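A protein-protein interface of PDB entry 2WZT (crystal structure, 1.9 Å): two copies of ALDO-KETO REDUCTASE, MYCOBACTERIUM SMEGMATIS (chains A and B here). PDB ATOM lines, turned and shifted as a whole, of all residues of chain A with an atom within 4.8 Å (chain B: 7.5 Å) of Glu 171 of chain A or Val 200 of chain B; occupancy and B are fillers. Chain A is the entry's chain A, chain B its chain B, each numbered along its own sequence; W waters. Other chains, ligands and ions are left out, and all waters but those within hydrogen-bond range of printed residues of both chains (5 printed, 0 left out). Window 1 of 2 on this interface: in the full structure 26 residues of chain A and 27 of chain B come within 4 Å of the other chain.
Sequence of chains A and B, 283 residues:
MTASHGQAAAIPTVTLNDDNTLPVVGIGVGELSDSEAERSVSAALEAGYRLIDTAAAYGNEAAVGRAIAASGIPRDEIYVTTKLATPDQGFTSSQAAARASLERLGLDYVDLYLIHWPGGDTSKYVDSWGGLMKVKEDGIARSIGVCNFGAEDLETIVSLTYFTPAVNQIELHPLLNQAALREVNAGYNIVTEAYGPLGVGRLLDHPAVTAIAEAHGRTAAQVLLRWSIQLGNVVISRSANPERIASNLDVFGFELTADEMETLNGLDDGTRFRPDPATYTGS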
ATOM      1  N   GLU A  31     -27.880   3.331  36.543  1.00  0.00           N
ATOM      2  CA  GLU A  31     -26.758   2.400  36.297  1.00  0.00           C
ATOM      3  C   GLU A  31     -25.974   1.996  37.547  1.00  0.00           C
ATOM      4  O   GLU A  31     -24.811   1.588  37.461  1.00  0.00           O
ATOM      5  CB  GLU A  31     -25.805   2.976  35.254  1.00  0.00           C
ATOM      6  CG  GLU A  31     -26.413   3.024  33.871  1.00  0.00           C
ATOM      7  CD  GLU A  31     -25.732   4.034  32.980  1.00  0.00           C
ATOM      8  OE1 GLU A  31     -25.586   5.202  33.406  1.00  0.00           O
ATOM      9  OE2 GLU A  31     -25.357   3.655  31.851  1.00  0.00           O
ATOM     10  N   ASN A 148     -38.109  13.597  28.959  1.00  0.00           N
ATOM     11  CA  ASN A 148     -37.833  13.552  27.529  1.00  0.00           C
ATOM     12  C   ASN A 148     -39.089  13.690  26.660  1.00  0.00           C
ATOM     13  O   ASN A 148     -39.220  13.033  25.637  1.00  0.00           O
ATOM     14  CB  ASN A 148     -36.996  12.298  27.168  1.00  0.00           C
ATOM     15  CG  ASN A 148     -35.549  12.434  27.601  1.00  0.00           C
ATOM     16  OD1 ASN A 148     -35.030  11.630  28.378  1.00  0.00           O
ATOM     17  ND2 ASN A 148     -34.900  13.467  27.117  1.00  0.00           N
ATOM     18  N   GLN A 169     -38.026  16.166  32.673  1.00  0.00           N
ATOM     19  CA  GLN A 169     -36.638  15.806  32.942  1.00  0.00           C
ATOM     20  C   GLN A 169     -35.888  15.396  31.648  1.00  0.00           C
ATOM     21  O   GLN A 169     -36.299  14.486  30.904  1.00  0.00           O
ATOM     22  CB  GLN A 169     -36.593  14.673  33.981  1.00  0.00           C
ATOM     23  CG  GLN A 169     -35.163  14.207  34.321  1.00  0.00           C
ATOM     24  CD  GLN A 169     -35.108  13.061  35.336  1.00  0.00           C
ATOM     25  OE1 GLN A 169     -35.654  13.142  36.466  1.00  0.00           O
ATOM     26  NE2 GLN A 169     -34.426  11.992  34.944  1.00  0.00           N
ATOM     27  N   ILE A 170     -34.778  16.082  31.380  1.00  0.00           N
ATOM     28  CA  ILE A 170     -34.036  15.889  30.121  1.00  0.00           C
ATOM     29  C   ILE A 170     -32.535  16.025  30.355  1.00  0.00           C
ATOM     30  O   ILE A 170     -32.119  16.620  31.343  1.00  0.00           O
ATOM     31  CB  ILE A 170     -34.459  16.939  29.034  1.00  0.00           C
ATOM     32  CG1 ILE A 170     -34.230  18.386  29.576  1.00  0.00           C
ATOM     33  CG2 ILE A 170     -35.909  16.734  28.591  1.00  0.00           C
ATOM     34  CD1 ILE A 170     -34.708  19.487  28.677  1.00  0.00           C
ATOM     35  N   GLU A 171     -31.723  15.472  29.454  1.00  0.00           N
ATOM     36  CA  GLU A 171     -30.283  15.704  29.499  1.00  0.00           C
ATOM     37  C   GLU A 171     -30.025  17.174  29.194  1.00  0.00           C
ATOM     38  O   GLU A 171     -30.615  17.713  28.245  1.00  0.00           O
ATOM     39  CB  GLU A 171     -29.554  14.827  28.464  1.00  0.00           C
ATOM     40  CG  GLU A 171     -28.034  14.844  28.704  1.00  0.00           C
ATOM     41  CD  GLU A 171     -27.216  14.171  27.610  1.00  0.00           C
ATOM     42  OE1 GLU A 171     -27.780  13.563  26.695  1.00  0.00           O
ATOM     43  OE2 GLU A 171     -25.984  14.293  27.655  1.00  0.00           O
ATOM     44  N   LEU A 172     -29.157  17.823  29.981  1.00  0.00           N
ATOM     45  CA  LEU A 172     -28.914  19.258  29.826  1.00  0.00           C
ATOM     46  C   LEU A 172     -27.566  19.656  30.430  1.00  0.00           C
ATOM     47  O   LEU A 172     -27.312  19.442  31.615  1.00  0.00           O
ATOM     48  CB  LEU A 172     -30.071  20.083  30.470  1.00  0.00           C
ATOM     49  CG  LEU A 172     -30.268  21.554  30.074  1.00  0.00           C
ATOM     50  CD1 LEU A 172     -31.680  21.988  30.503  1.00  0.00           C
ATOM     51  CD2 LEU A 172     -29.203  22.461  30.721  1.00  0.00           C
ATOM     52  N   HIS A 173     -26.696  20.209  29.586  1.00  0.00           N
ATOM     53  CA  HIS A 173     -25.391  20.704  30.017  1.00  0.00           C
ATOM     54  C   HIS A 173     -25.005  21.781  28.995  1.00  0.00           C
ATOM     55  O   HIS A 173     -25.734  21.969  28.023  1.00  0.00           O
ATOM     56  CB  HIS A 173     -24.349  19.564  30.123  1.00  0.00           C
ATOM     57  CG  HIS A 173     -24.208  18.729  28.880  1.00  0.00           C
ATOM     58  ND1 HIS A 173     -23.533  19.172  27.762  1.00  0.00           N
ATOM     59  CD2 HIS A 173     -24.636  17.476  28.583  1.00  0.00           C
ATOM     60  CE1 HIS A 173     -23.544  18.228  26.834  1.00  0.00           C
ATOM     61  NE2 HIS A 173     -24.214  17.192  27.302  1.00  0.00           N
ATOM     62  N   LEU A 176     -25.335  21.097  25.396  1.00  0.00           N
ATOM     63  CA  LEU A 176     -26.683  20.632  25.078  1.00  0.00           C
ATOM     64  C   LEU A 176     -27.628  21.378  26.033  1.00  0.00           C
ATOM     65  O   LEU A 176     -28.207  20.785  26.954  1.00  0.00           O
ATOM     66  CB  LEU A 176     -26.824  19.114  25.284  1.00  0.00           C
ATOM     67  CG  LEU A 176     -28.174  18.438  24.926  1.00  0.00           C
ATOM     68  CD1 LEU A 176     -28.514  18.632  23.461  1.00  0.00           C
ATOM     69  CD2 LEU A 176     -28.182  16.927  25.288  1.00  0.00           C
ATOM     70  N   GLN A 178     -30.451  22.914  25.796  1.00  0.00           N
ATOM     71  CA  GLN A 178     -31.921  22.777  25.713  1.00  0.00           C
ATOM     72  C   GLN A 178     -32.667  24.111  25.830  1.00  0.00           C
ATOM     73  O   GLN A 178     -33.775  24.155  26.364  1.00  0.00           O
ATOM     74  CB  GLN A 178     -32.436  21.804  26.808  1.00  0.00           C
ATOM     75  CG  GLN A 178     -31.733  20.418  26.783  1.00  0.00           C
ATOM     76  CD  GLN A 178     -32.310  19.464  25.746  1.00  0.00           C
ATOM     77  OE1 GLN A 178     -32.934  19.883  24.768  1.00  0.00           O
ATOM     78  NE2 GLN A 178     -32.089  18.165  25.952  1.00  0.00           N
ATOM     79  N   TYR A 195     -30.375  16.404  33.765  1.00  0.00           N
ATOM     80  CA  TYR A 195     -29.460  15.336  34.160  1.00  0.00           C
ATOM     81  C   TYR A 195     -28.286  15.296  33.175  1.00  0.00           C
ATOM     82  O   TYR A 195     -28.332  15.956  32.139  1.00  0.00           O
ATOM     83  CB  TYR A 195     -30.181  13.956  34.277  1.00  0.00           C
ATOM     84  CG  TYR A 195     -30.740  13.387  32.975  1.00  0.00           C
ATOM     85  CD1 TYR A 195     -29.903  12.718  32.048  1.00  0.00           C
ATOM     86  CD2 TYR A 195     -32.098  13.522  32.665  1.00  0.00           C
ATOM     87  CE1 TYR A 195     -30.420  12.192  30.836  1.00  0.00           C
ATOM     88  CE2 TYR A 195     -32.630  13.002  31.473  1.00  0.00           C
ATOM     89  CZ  TYR A 195     -31.791  12.349  30.555  1.00  0.00           C
ATOM     90  OH  TYR A 195     -32.359  11.849  29.383  1.00  0.00           O
ATOM     91  N   GLY A 196     -27.237  14.557  33.525  1.00  0.00           N
ATOM     92  CA  GLY A 196     -25.950  14.612  32.821  1.00  0.00           C
ATOM     93  C   GLY A 196     -25.344  16.038  32.776  1.00  0.00           C
ATOM     94  O   GLY A 196     -24.875  16.455  31.721  1.00  0.00           O
ATOM     95  N   ARG A 238     -25.135  12.765  38.776  1.00  0.00           N
ATOM     96  CA  ARG A 238     -24.855  11.321  38.774  1.00  0.00           C
ATOM     97  C   ARG A 238     -24.119  10.982  40.062  1.00  0.00           C
ATOM     98  O   ARG A 238     -23.340  11.784  40.582  1.00  0.00           O
ATOM     99  CB  ARG A 238     -23.961  10.904  37.593  1.00  0.00           C
ATOM    100  CG  ARG A 238     -24.513  11.101  36.171  1.00  0.00           C
ATOM    101  CD  ARG A 238     -23.616  10.353  35.139  1.00  0.00           C
ATOM    102  NE  ARG A 238     -23.663   8.909  35.366  1.00  0.00           N
ATOM    103  CZ  ARG A 238     -23.934   7.959  34.459  1.00  0.00           C
ATOM    104  NH1 ARG A 238     -24.153   8.239  33.183  1.00  0.00           N
ATOM    105  NH2 ARG A 238     -23.954   6.689  34.839  1.00  0.00           N
ATOM    106  N   GLU B 171     -20.022  13.446  22.003  1.00  0.00           N
ATOM    107  CA  GLU B 171     -21.116  12.737  22.671  1.00  0.00           C
ATOM    108  C   GLU B 171     -22.097  12.340  21.597  1.00  0.00           C
ATOM    109  O   GLU B 171     -22.475  13.181  20.764  1.00  0.00           O
ATOM    110  CB  GLU B 171     -21.834  13.592  23.713  1.00  0.00           C
ATOM    111  CG  GLU B 171     -22.819  12.753  24.551  1.00  0.00           C
ATOM    112  CD  GLU B 171     -23.732  13.584  25.469  1.00  0.00           C
ATOM    113  OE1 GLU B 171     -23.535  14.824  25.583  1.00  0.00           O
ATOM    114  OE2 GLU B 171     -24.655  12.979  26.073  1.00  0.00           O
ATOM    115  N   HIS B 173     -25.516   9.509  20.883  1.00  0.00           N
ATOM    116  CA  HIS B 173     -26.461   8.433  21.216  1.00  0.00           C
ATOM    117  C   HIS B 173     -27.754   8.716  20.443  1.00  0.00           C
ATOM    118  O   HIS B 173     -27.877   9.786  19.817  1.00  0.00           O
ATOM    119  CB  HIS B 173     -26.669   8.314  22.752  1.00  0.00           C
ATOM    120  CG  HIS B 173     -27.120   9.587  23.403  1.00  0.00           C
ATOM    121  ND1 HIS B 173     -28.413  10.051  23.308  1.00  0.00           N
ATOM    122  CD2 HIS B 173     -26.455  10.482  24.172  1.00  0.00           C
ATOM    123  CE1 HIS B 173     -28.531  11.181  23.992  1.00  0.00           C
ATOM    124  NE2 HIS B 173     -27.361  11.448  24.553  1.00  0.00           N
ATOM    125  N   LEU B 175     -30.521   9.878  21.079  1.00  0.00           N
ATOM    126  CA  LEU B 175     -31.193  11.171  21.316  1.00  0.00           C
ATOM    127  C   LEU B 175     -30.321  12.351  20.943  1.00  0.00           C
ATOM    128  O   LEU B 175     -30.733  13.514  21.052  1.00  0.00           O
ATOM    129  CB  LEU B 175     -31.738  11.320  22.755  1.00  0.00           C
ATOM    130  CG  LEU B 175     -33.262  11.400  22.849  1.00  0.00           C
ATOM    131  CD1 LEU B 175     -33.921  10.063  22.502  1.00  0.00           C
ATOM    132  CD2 LEU B 175     -33.736  11.881  24.229  1.00  0.00           C
ATOM    133  N   LEU B 176     -29.126  12.041  20.480  1.00  0.00           N
ATOM    134  CA  LEU B 176     -28.135  13.063  20.082  1.00  0.00           C
ATOM    135  C   LEU B 176     -27.269  12.392  19.029  1.00  0.00           C
ATOM    136  O   LEU B 176     -26.111  12.011  19.287  1.00  0.00           O
ATOM    137  CB  LEU B 176     -27.299  13.504  21.305  1.00  0.00           C
ATOM    138  CG  LEU B 176     -26.228  14.597  21.110  1.00  0.00           C
ATOM    139  CD1 LEU B 176     -26.874  15.871  20.598  1.00  0.00           C
ATOM    140  CD2 LEU B 176     -25.420  14.828  22.421  1.00  0.00           C
ATOM    141  N   GLY B 196     -20.620   8.489  25.724  1.00  0.00           N
ATOM    142  CA  GLY B 196     -21.982   8.596  26.276  1.00  0.00           C
ATOM    143  C   GLY B 196     -23.029   7.828  25.428  1.00  0.00           C
ATOM    144  O   GLY B 196     -24.151   8.328  25.226  1.00  0.00           O
ATOM    145  N   PRO B 197     -22.694   6.598  24.949  1.00  0.00           N
ATOM    146  CA  PRO B 197     -23.607   5.866  24.020  1.00  0.00           C
ATOM    147  C   PRO B 197     -24.965   5.465  24.650  1.00  0.00           C
ATOM    148  O   PRO B 197     -25.932   5.127  23.927  1.00  0.00           O
ATOM    149  CB  PRO B 197     -22.786   4.623  23.633  1.00  0.00           C
ATOM    150  CG  PRO B 197     -21.890   4.378  24.818  1.00  0.00           C
ATOM    151  CD  PRO B 197     -21.478   5.797  25.231  1.00  0.00           C
ATOM    152  N   LEU B 198     -25.052   5.524  25.985  1.00  0.00           N
ATOM    153  CA  LEU B 198     -26.294   5.149  26.653  1.00  0.00           C
ATOM    154  C   LEU B 198     -27.180   6.326  27.123  1.00  0.00           C
ATOM    155  O   LEU B 198     -28.185   6.101  27.805  1.00  0.00           O
ATOM    156  CB  LEU B 198     -26.011   4.170  27.819  1.00  0.00           C
ATOM    157  CG  LEU B 198     -24.991   3.039  27.588  1.00  0.00           C
ATOM    158  CD1 LEU B 198     -24.842   2.188  28.837  1.00  0.00           C
ATOM    159  CD2 LEU B 198     -25.401   2.158  26.393  1.00  0.00           C
ATOM    160  N   GLY B 199     -26.808   7.565  26.804  1.00  0.00           N
ATOM    161  CA  GLY B 199     -27.662   8.732  27.180  1.00  0.00           C
ATOM    162  C   GLY B 199     -27.875   8.849  28.679  1.00  0.00           C
ATOM    163  O   GLY B 199     -28.999   9.031  29.165  1.00  0.00           O
ATOM    164  N   VAL B 200     -26.784   8.716  29.433  1.00  0.00           N
ATOM    165  CA  VAL B 200     -26.819   8.852  30.911  1.00  0.00           C
ATOM    166  C   VAL B 200     -27.707   7.752  31.531  1.00  0.00           C
ATOM    167  O   VAL B 200     -28.391   7.947  32.550  1.00  0.00           O
ATOM    168  CB  VAL B 200     -27.222  10.310  31.358  1.00  0.00           C
ATOM    169  CG1 VAL B 200     -26.735  10.610  32.783  1.00  0.00           C
ATOM    170  CG2 VAL B 200     -26.656  11.373  30.381  1.00  0.00           C
ATOM    171  N   GLY B 201     -27.715   6.601  30.864  1.00  0.00           N
ATOM    172  CA  GLY B 201     -28.453   5.434  31.310  1.00  0.00           C
ATOM    173  C   GLY B 201     -29.901   5.372  30.868  1.00  0.00           C
ATOM    174  O   GLY B 201     -30.515   4.309  30.941  1.00  0.00           O
ATOM    175  N   ARG B 202     -30.470   6.506  30.434  1.00  0.00           N
ATOM    176  CA  ARG B 202     -31.920   6.564  30.117  1.00  0.00           C
ATOM    177  C   ARG B 202     -32.379   5.697  28.942  1.00  0.00           C
ATOM    178  O   ARG B 202     -33.493   5.164  28.971  1.00  0.00           O
ATOM    179  CB  ARG B 202     -32.358   8.008  29.871  1.00  0.00           C
ATOM    180  CG  ARG B 202     -32.745   8.753  31.131  1.00  0.00           C
ATOM    181  CD  ARG B 202     -31.528   9.010  32.025  1.00  0.00           C
ATOM    182  NE  ARG B 202     -31.908   9.831  33.176  1.00  0.00           N
ATOM    183  CZ  ARG B 202     -31.107  10.140  34.191  1.00  0.00           C
ATOM    184  NH1 ARG B 202     -29.838   9.712  34.219  1.00  0.00           N
ATOM    185  NH2 ARG B 202     -31.581  10.882  35.180  1.00  0.00           N
ATOM    186  N   LEU B 203     -31.504   5.545  27.940  1.00  0.00           N
ATOM    187  CA  LEU B 203     -31.877   4.860  26.695  1.00  0.00           C
ATOM    188  C   LEU B 203     -31.995   3.354  26.889  1.00  0.00           C
ATOM    189  O   LEU B 203     -32.584   2.658  26.048  1.00  0.00           O
ATOM    190  CB  LEU B 203     -30.903   5.196  25.562  1.00  0.00           C
ATOM    191  CG  LEU B 203     -31.060   6.633  25.033  1.00  0.00           C
ATOM    192  CD1 LEU B 203     -29.755   7.139  24.483  1.00  0.00           C
ATOM    193  CD2 LEU B 203     -32.186   6.737  23.994  1.00  0.00           C
ATOM    194  N   LEU B 204     -31.476   2.857  28.010  1.00  0.00           N
ATOM    195  CA  LEU B 204     -31.627   1.428  28.339  1.00  0.00           C
ATOM    196  C   LEU B 204     -33.101   1.043  28.536  1.00  0.00           C
ATOM    197  O   LEU B 204     -33.466  -0.129  28.399  1.00  0.00           O
ATOM    198  CB  LEU B 204     -30.812   1.061  29.581  1.00  0.00           C
ATOM    199  CG  LEU B 204     -29.311   1.392  29.565  1.00  0.00           C
ATOM    200  CD1 LEU B 204     -28.717   1.205  30.968  1.00  0.00           C
ATOM    201  CD2 LEU B 204     -28.540   0.559  28.590  1.00  0.00           C
ATOM    202  N   ARG B 238     -18.412   3.947  28.932  1.00  0.00           N
ATOM    203  CA  ARG B 238     -17.950   4.274  30.271  1.00  0.00           C
ATOM    204  C   ARG B 238     -17.763   2.981  31.069  1.00  0.00           C
ATOM    205  O   ARG B 238     -18.348   1.941  30.760  1.00  0.00           O
ATOM    206  CB  ARG B 238     -18.974   5.123  31.015  1.00  0.00           C
ATOM    207  CG  ARG B 238     -19.773   6.127  30.196  1.00  0.00           C
ATOM    208  CD  ARG B 238     -20.896   6.698  31.083  1.00  0.00           C
ATOM    209  NE  ARG B 238     -20.350   7.261  32.319  1.00  0.00           N
ATOM    210  CZ  ARG B 238     -20.511   6.738  33.534  1.00  0.00           C
ATOM    211  NH1 ARG B 238     -21.231   5.631  33.708  1.00  0.00           N
ATOM    212  NH2 ARG B 238     -19.951   7.336  34.589  1.00  0.00           N
HETATM  213  O   HOH W   1     -27.370   6.939  34.804  1.00  0.00           O
HETATM  214  O   HOH W   2     -24.457   6.022  31.063  1.00  0.00           O
HETATM  215  O   HOH W   3     -34.859  10.419  32.870  1.00  0.00           O
HETATM  216  O   HOH W   4     -30.929  10.488  27.797  1.00  0.00           O
HETATM  217  O   HOH W   5     -22.639   3.483  32.087  1.00  0.00           O
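The side-chain amide nitrogen (NE2) of Gln 169 of chain A lies close to the guanidinium group (NH2) of Arg 202 of chain B (3.1 Å).
The guanidinium group (NH2) of Arg 238 of chain A sits close to the guanidinium group (NH1) of Arg 238 of chain B (3.1 Å).
A ring nitrogen (NE2) of His 173 of chain A sits at hydrogen-bond distance from the side-chain carboxylate (OE1) of Glu 171 of chain B (3.0 Å).
OE1 of Glu 171 of chain A is in hydrogen-bond range of NE2 of His 173 of chain B (3.0 Å).
OE2 of Glu 171 of chain B sits close to OE2 of Glu 171 of chain A (2.4 Å).
The side-chain carboxylate (OE1) of Glu 31 of chain A is in salt-bridge range of the guanidinium group (NH2) of Arg 238 of chain A (2.6 Å).
The side-chain carboxylate (OE2) of Glu 171 of chain A sits at hydrogen-bond distance from a ring nitrogen (NE2) of His 173 of chain A (3.4 Å).
The side-chain carboxylate (OE2) of Glu 171 of chain B is in hydrogen-bond range of a ring nitrogen (NE2) of His 173 of chain B, at 3.5 Å.
O of Leu 198 of chain B lies within hydrogen-bond range of N of Leu 203 of chain B, at 3.4 Å.
A ring nitrogen (ND1) of His 173 of chain B sits close to the backbone NH (N) of Leu 175 of chain B, at 3.1 Å.
N of Leu 172 of chain A is in hydrogen-bond range of O of Tyr 195 of chain A, 3.0 Å away.
Among the printed residues, merely in contact across the chains: Glu 31 of chain A with Leu 198 of chain B, Tyr 195 of chain A with Arg 202 of chain B, Glu 31 of chain A with Gly 201 of chain B, Asn 148 of chain A with Leu 175 of chain B, Arg 238 of chain A with Val 200 of chain B, Tyr 195 of chain A with Val 200 of chain B, Glu 31 of chain A with Val 200 of chain B, Tyr 195 of chain A with Gly 199 of chain B and Glu 171 of chain A with Val 200 of chain B.
Glu 171 of chain A touches three residues of chain B.
Printed residues of chain A within 4 Å of Val 200 of chain B: Glu 31 (3.8 Å), Glu 171 (3.98 Å), Tyr 195 (3.7 Å) and Arg 238 (3.5 Å).
Printed residues of chain A within 4 Å of Arg 238 of chain B: Arg 238.
Of the printed residues of chain B, Gln 169 of chain A touches Arg 202.
Printed residues of chain B within 4 Å of His 173 of chain A: Glu 171 (3.0 Å).
Printed residues of chain A within 4 Å of Gly 201 of chain B: Glu 31.
Printed residues of chain A within 4 Å of His 173 of chain B: Glu 171 (3.0 Å).
The nearest residue of chain B that does not touch Glu 171 of chain A is Gly 199 of chain B (4.9 Å).
The nearest printed residue of chain A that does not touch Val 200 of chain B is Gly 196 of chain A (4.05 Å).
Of the 12 printed residues of chain A, 7 touch a printed residue of chain B.
Printed residues of chain A that touch a printed residue of chain B: Glu 31, Asn 148, Gln 169, Glu 171, His 173, Tyr 195 and Arg 238.
Of the 14 printed residues of chain B, 9 touch a printed residue of chain A.
Among the printed residues, 14 pairs touch across the chains.
Among the printed residues, no Asp or Glu carboxylate lies within 4 Å of a Lys or Arg side-chain nitrogen of the other chain.
Glu 171 of chain B touches its own counterpart, Glu 171 of chain A.
Glu 171 of chain A touches His 173 of chain B, and with the chains exchanged His 173 of chain A touches Glu 171 of chain B.
Arg 238 of chain B touches its own counterpart, Arg 238 of chain A.
5 positions are printed for both chains.
Of the 14 pairs that touch across the chains among the printed residues, 4 have their exchanged pair printed and touching as well.
Water W4 lies within hydrogen-bond range of OH of Tyr 195 of chain A (2.5 Å) and O of Gly 199 of chain B (2.8 Å).
Water W3 bridges NE2 of Gln 169 of chain A (2.6 Å) and NE of Arg 202 of chain B (3.0 Å).
Water W2 lies within hydrogen-bond range of OE2 of Glu 31 of chain A (2.7 Å), NH1 of Arg 238 of chain A (3.1 Å) and N of Gly 201 of chain B (3.3 Å).
Water W1 lies within hydrogen-bond range of O of Val 200 of chain B (2.7 Å), OE1 of Glu 31 of chain A (2.9 Å) and NH2 of Arg 238 of chain A (3.4 Å).
Water W5 lies within hydrogen-bond range of the side-chain carboxylate of Glu 31 of chain A (2.7 Å) and the guanidinium group of Arg 238 of chain B (3.0 Å).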
